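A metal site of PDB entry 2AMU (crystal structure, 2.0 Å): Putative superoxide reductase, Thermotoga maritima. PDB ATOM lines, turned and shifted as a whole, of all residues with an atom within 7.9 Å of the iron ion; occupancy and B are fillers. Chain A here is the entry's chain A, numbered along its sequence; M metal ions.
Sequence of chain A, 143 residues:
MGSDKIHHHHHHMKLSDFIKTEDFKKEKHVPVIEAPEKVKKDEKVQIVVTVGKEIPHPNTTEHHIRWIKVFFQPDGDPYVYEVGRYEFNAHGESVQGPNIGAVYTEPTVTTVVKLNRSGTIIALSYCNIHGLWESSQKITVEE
The side-chain sulfur of Cys 127 lies close to the backbone carbonyl oxygen of His 64 (3.7 Å). The side-chain sulfur (SG) of Cys 127 sits close to the backbone NH (N) of Ile 129. NE1 of Trp 133 lies within hydrogen-bond range of O of His 130, 2.9 Å away. A ring nitrogen (ND1) of His 29 sits at hydrogen-bond distance from the side-chain carboxylate of Glu 27.
Of the 16 residues printed, 5 come within 4 Å of the iron ion.
The iron ion is bound by NE2 of His 29, NE2 of His 57, ND1 of His 130, NE2 of His 63 and SG of Cys 127.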
ATOM      1  N   GLU A  27     -11.857 -22.923   0.216  1.00  0.00           N
ATOM      2  CA  GLU A  27     -12.284 -21.523   0.077  1.00  0.00           C
ATOM      3  C   GLU A  27     -13.255 -21.274  -1.111  1.00  0.00           C
ATOM      4  O   GLU A  27     -12.853 -21.346  -2.276  1.00  0.00           O
ATOM      5  CB  GLU A  27     -11.031 -20.612  -0.059  1.00  0.00           C
ATOM      6  CG  GLU A  27     -11.351 -19.105  -0.212  1.00  0.00           C
ATOM      7  CD  GLU A  27     -12.361 -18.595   0.810  1.00  0.00           C
ATOM      8  OE1 GLU A  27     -12.061 -18.665   2.010  1.00  0.00           O
ATOM      9  OE2 GLU A  27     -13.471 -18.128   0.445  1.00  0.00           O
ATOM     10  N   LYS A  28     -14.526 -20.953  -0.783  1.00  0.00           N
ATOM     11  CA  LYS A  28     -15.573 -20.622  -1.797  1.00  0.00           C
ATOM     12  C   LYS A  28     -15.220 -19.491  -2.756  1.00  0.00           C
ATOM     13  O   LYS A  28     -15.730 -19.423  -3.847  1.00  0.00           O
ATOM     14  CB  LYS A  28     -16.937 -20.294  -1.119  1.00  0.00           C
ATOM     15  CG  LYS A  28     -16.962 -19.055  -0.164  1.00  0.00           C
ATOM     16  CD  LYS A  28     -18.344 -18.911   0.562  1.00  0.00           C
ATOM     17  CE  LYS A  28     -18.219 -18.523   2.066  1.00  0.00           C
ATOM     18  NZ  LYS A  28     -19.092 -19.356   3.019  1.00  0.00           N
ATOM     19  N   HIS A  29     -14.357 -18.573  -2.321  1.00  0.00           N
ATOM     20  CA  HIS A  29     -14.076 -17.403  -3.097  1.00  0.00           C
ATOM     21  C   HIS A  29     -13.106 -17.609  -4.245  1.00  0.00           C
ATOM     22  O   HIS A  29     -13.092 -16.806  -5.159  1.00  0.00           O
ATOM     23  CB  HIS A  29     -13.561 -16.289  -2.192  1.00  0.00           C
ATOM     24  CG  HIS A  29     -14.632 -15.647  -1.348  1.00  0.00           C
ATOM     25  ND1 HIS A  29     -14.767 -15.904   0.001  1.00  0.00           N
ATOM     26  CD2 HIS A  29     -15.578 -14.734  -1.662  1.00  0.00           C
ATOM     27  CE1 HIS A  29     -15.755 -15.171   0.483  1.00  0.00           C
ATOM     28  NE2 HIS A  29     -16.276 -14.466  -0.517  1.00  0.00           N
ATOM     29  N   VAL A  51     -16.674 -19.335  -9.595  1.00  0.00           N
ATOM     30  CA  VAL A  51     -16.481 -19.057  -8.174  1.00  0.00           C
ATOM     31  C   VAL A  51     -17.577 -19.803  -7.479  1.00  0.00           C
ATOM     32  O   VAL A  51     -18.732 -19.749  -7.870  1.00  0.00           O
ATOM     33  CB  VAL A  51     -16.537 -17.544  -7.803  1.00  0.00           C
ATOM     34  CG1 VAL A  51     -16.556 -17.340  -6.230  1.00  0.00           C
ATOM     35  CG2 VAL A  51     -15.371 -16.825  -8.429  1.00  0.00           C
ATOM     36  N   HIS A  57     -21.050 -19.896  -3.016  1.00  0.00           N
ATOM     37  CA  HIS A  57     -20.927 -18.562  -2.499  1.00  0.00           C
ATOM     38  C   HIS A  57     -22.306 -17.890  -2.657  1.00  0.00           C
ATOM     39  O   HIS A  57     -22.962 -18.086  -3.698  1.00  0.00           O
ATOM     40  CB  HIS A  57     -19.834 -17.817  -3.283  1.00  0.00           C
ATOM     41  CG  HIS A  57     -19.625 -16.415  -2.823  1.00  0.00           C
ATOM     42  ND1 HIS A  57     -20.524 -15.408  -3.086  1.00  0.00           N
ATOM     43  CD2 HIS A  57     -18.637 -15.866  -2.086  1.00  0.00           C
ATOM     44  CE1 HIS A  57     -20.109 -14.283  -2.530  1.00  0.00           C
ATOM     45  NE2 HIS A  57     -18.960 -14.540  -1.914  1.00  0.00           N
ATOM     46  N   PRO A  58     -22.736 -17.080  -1.662  1.00  0.00           N
ATOM     47  CA  PRO A  58     -24.025 -16.371  -1.731  1.00  0.00           C
ATOM     48  C   PRO A  58     -24.202 -15.516  -2.968  1.00  0.00           C
ATOM     49  O   PRO A  58     -23.216 -15.016  -3.527  1.00  0.00           O
ATOM     50  CB  PRO A  58     -23.981 -15.453  -0.497  1.00  0.00           C
ATOM     51  CG  PRO A  58     -23.119 -16.175   0.469  1.00  0.00           C
ATOM     52  CD  PRO A  58     -22.024 -16.751  -0.414  1.00  0.00           C
ATOM     53  N   HIS A  63     -24.490  -9.227  -0.916  1.00  0.00           N
ATOM     54  CA  HIS A  63     -23.268 -10.031  -0.925  1.00  0.00           C
ATOM     55  C   HIS A  63     -23.247 -10.902  -2.196  1.00  0.00           C
ATOM     56  O   HIS A  63     -24.077 -11.768  -2.410  1.00  0.00           O
ATOM     57  CB  HIS A  63     -23.194 -10.867   0.364  1.00  0.00           C
ATOM     58  CG  HIS A  63     -22.012 -11.766   0.442  1.00  0.00           C
ATOM     59  ND1 HIS A  63     -21.991 -12.893   1.234  1.00  0.00           N
ATOM     60  CD2 HIS A  63     -20.803 -11.714  -0.168  1.00  0.00           C
ATOM     61  CE1 HIS A  63     -20.822 -13.496   1.106  1.00  0.00           C
ATOM     62  NE2 HIS A  63     -20.088 -12.803   0.254  1.00  0.00           N
ATOM     63  N   HIS A  64     -22.273 -10.660  -3.051  1.00  0.00           N
ATOM     64  CA  HIS A  64     -22.218 -11.391  -4.324  1.00  0.00           C
ATOM     65  C   HIS A  64     -20.866 -11.239  -4.949  1.00  0.00           C
ATOM     66  O   HIS A  64     -20.143 -10.288  -4.644  1.00  0.00           O
ATOM     67  CB  HIS A  64     -23.285 -10.856  -5.300  1.00  0.00           C
ATOM     68  CG  HIS A  64     -23.285  -9.358  -5.452  1.00  0.00           C
ATOM     69  ND1 HIS A  64     -24.199  -8.547  -4.816  1.00  0.00           N
ATOM     70  CD2 HIS A  64     -22.478  -8.533  -6.159  1.00  0.00           C
ATOM     71  CE1 HIS A  64     -23.956  -7.289  -5.135  1.00  0.00           C
ATOM     72  NE2 HIS A  64     -22.917  -7.256  -5.949  1.00  0.00           N
ATOM     73  N   ILE A  65     -20.570 -12.136  -5.898  1.00  0.00           N
ATOM     74  CA  ILE A  65     -19.394 -12.046  -6.759  1.00  0.00           C
ATOM     75  C   ILE A  65     -19.741 -11.096  -7.900  1.00  0.00           C
ATOM     76  O   ILE A  65     -20.734 -11.260  -8.586  1.00  0.00           O
ATOM     77  CB  ILE A  65     -18.942 -13.439  -7.273  1.00  0.00           C
ATOM     78  CG1 ILE A  65     -18.622 -14.371  -6.101  1.00  0.00           C
ATOM     79  CG2 ILE A  65     -17.771 -13.340  -8.271  1.00  0.00           C
ATOM     80  CD1 ILE A  65     -17.489 -13.913  -5.161  1.00  0.00           C
ATOM     81  N   TYR A 126     -13.610 -10.968  -7.929  1.00  0.00           N
ATOM     82  CA  TYR A 126     -13.871  -9.896  -7.003  1.00  0.00           C
ATOM     83  C   TYR A 126     -15.235 -10.149  -6.333  1.00  0.00           C
ATOM     84  O   TYR A 126     -16.252 -10.289  -7.010  1.00  0.00           O
ATOM     85  CB  TYR A 126     -13.835  -8.535  -7.726  1.00  0.00           C
ATOM     86  CG  TYR A 126     -14.166  -7.393  -6.771  1.00  0.00           C
ATOM     87  CD1 TYR A 126     -13.338  -7.111  -5.702  1.00  0.00           C
ATOM     88  CD2 TYR A 126     -15.311  -6.632  -6.918  1.00  0.00           C
ATOM     89  CE1 TYR A 126     -13.639  -6.089  -4.796  1.00  0.00           C
ATOM     90  CE2 TYR A 126     -15.632  -5.596  -6.013  1.00  0.00           C
ATOM     91  CZ  TYR A 126     -14.796  -5.332  -4.965  1.00  0.00           C
ATOM     92  OH  TYR A 126     -15.098  -4.284  -4.082  1.00  0.00           O
ATOM     93  N   CYS A 127     -15.250 -10.205  -5.009  1.00  0.00           N
ATOM     94  CA  CYS A 127     -16.465 -10.226  -4.242  1.00  0.00           C
ATOM     95  C   CYS A 127     -16.724  -8.809  -3.727  1.00  0.00           C
ATOM     96  O   CYS A 127     -15.786  -8.116  -3.330  1.00  0.00           O
ATOM     97  CB  CYS A 127     -16.361 -11.219  -3.077  1.00  0.00           C
ATOM     98  SG  CYS A 127     -17.788 -11.132  -1.938  1.00  0.00           S
ATOM     99  N   ASN A 128     -17.985  -8.374  -3.749  1.00  0.00           N
ATOM    100  CA  ASN A 128     -18.353  -7.038  -3.242  1.00  0.00           C
ATOM    101  C   ASN A 128     -17.982  -6.750  -1.782  1.00  0.00           C
ATOM    102  O   ASN A 128     -17.923  -5.595  -1.445  1.00  0.00           O
ATOM    103  CB  ASN A 128     -19.838  -6.663  -3.520  1.00  0.00           C
ATOM    104  CG  ASN A 128     -20.818  -7.316  -2.579  1.00  0.00           C
ATOM    105  OD1 ASN A 128     -20.600  -8.441  -2.175  1.00  0.00           O
ATOM    106  ND2 ASN A 128     -21.886  -6.600  -2.190  1.00  0.00           N
ATOM    107  N   ILE A 129     -17.738  -7.762  -0.949  1.00  0.00           N
ATOM    108  CA  ILE A 129     -17.341  -7.550   0.450  1.00  0.00           C
ATOM    109  C   ILE A 129     -16.075  -8.273   0.904  1.00  0.00           C
ATOM    110  O   ILE A 129     -15.521  -7.946   1.957  1.00  0.00           O
ATOM    111  CB  ILE A 129     -18.494  -7.828   1.446  1.00  0.00           C
ATOM    112  CG1 ILE A 129     -18.972  -9.270   1.371  1.00  0.00           C
ATOM    113  CG2 ILE A 129     -19.640  -6.915   1.115  1.00  0.00           C
ATOM    114  CD1 ILE A 129     -20.043  -9.652   2.489  1.00  0.00           C
ATOM    115  N   HIS A 130     -15.599  -9.230   0.123  1.00  0.00           N
ATOM    116  CA  HIS A 130     -14.473 -10.070   0.520  1.00  0.00           C
ATOM    117  C   HIS A 130     -13.319  -9.930  -0.413  1.00  0.00           C
ATOM    118  O   HIS A 130     -12.474 -10.798  -0.469  1.00  0.00           O
ATOM    119  CB  HIS A 130     -14.878 -11.554   0.577  1.00  0.00           C
ATOM    120  CG  HIS A 130     -15.808 -11.881   1.699  1.00  0.00           C
ATOM    121  ND1 HIS A 130     -17.045 -12.424   1.508  1.00  0.00           N
ATOM    122  CD2 HIS A 130     -15.676 -11.698   3.034  1.00  0.00           C
ATOM    123  CE1 HIS A 130     -17.642 -12.587   2.679  1.00  0.00           C
ATOM    124  NE2 HIS A 130     -16.823 -12.182   3.617  1.00  0.00           N
ATOM    125  N   GLY A 131     -13.264  -8.836  -1.168  1.00  0.00           N
ATOM    126  CA  GLY A 131     -12.117  -8.590  -2.001  1.00  0.00           C
ATOM    127  C   GLY A 131     -11.815  -9.501  -3.190  1.00  0.00           C
ATOM    128  O   GLY A 131     -12.718 -10.158  -3.791  1.00  0.00           O
ATOM    129  N   TRP A 133      -9.466 -12.400  -5.396  1.00  0.00           N
ATOM    130  CA  TRP A 133      -9.050 -13.802  -5.241  1.00  0.00           C
ATOM    131  C   TRP A 133      -8.505 -14.227  -6.590  1.00  0.00           C
ATOM    132  O   TRP A 133      -8.950 -13.716  -7.576  1.00  0.00           O
ATOM    133  CB  TRP A 133     -10.233 -14.671  -4.870  1.00  0.00           C
ATOM    134  CG  TRP A 133     -10.791 -14.288  -3.558  1.00  0.00           C
ATOM    135  CD1 TRP A 133     -11.693 -13.283  -3.312  1.00  0.00           C
ATOM    136  CD2 TRP A 133     -10.464 -14.856  -2.292  1.00  0.00           C
ATOM    137  NE1 TRP A 133     -11.957 -13.223  -1.968  1.00  0.00           N
ATOM    138  CE2 TRP A 133     -11.178 -14.154  -1.318  1.00  0.00           C
ATOM    139  CE3 TRP A 133      -9.614 -15.906  -1.883  1.00  0.00           C
ATOM    140  CZ2 TRP A 133     -11.107 -14.468   0.010  1.00  0.00           C
ATOM    141  CZ3 TRP A 133      -9.516 -16.182  -0.558  1.00  0.00           C
ATOM    142  CH2 TRP A 133     -10.262 -15.485   0.369  1.00  0.00           C
HETATM  143 FE    FE M   1     -17.874 -13.067  -0.563  1.00  0.00          FE
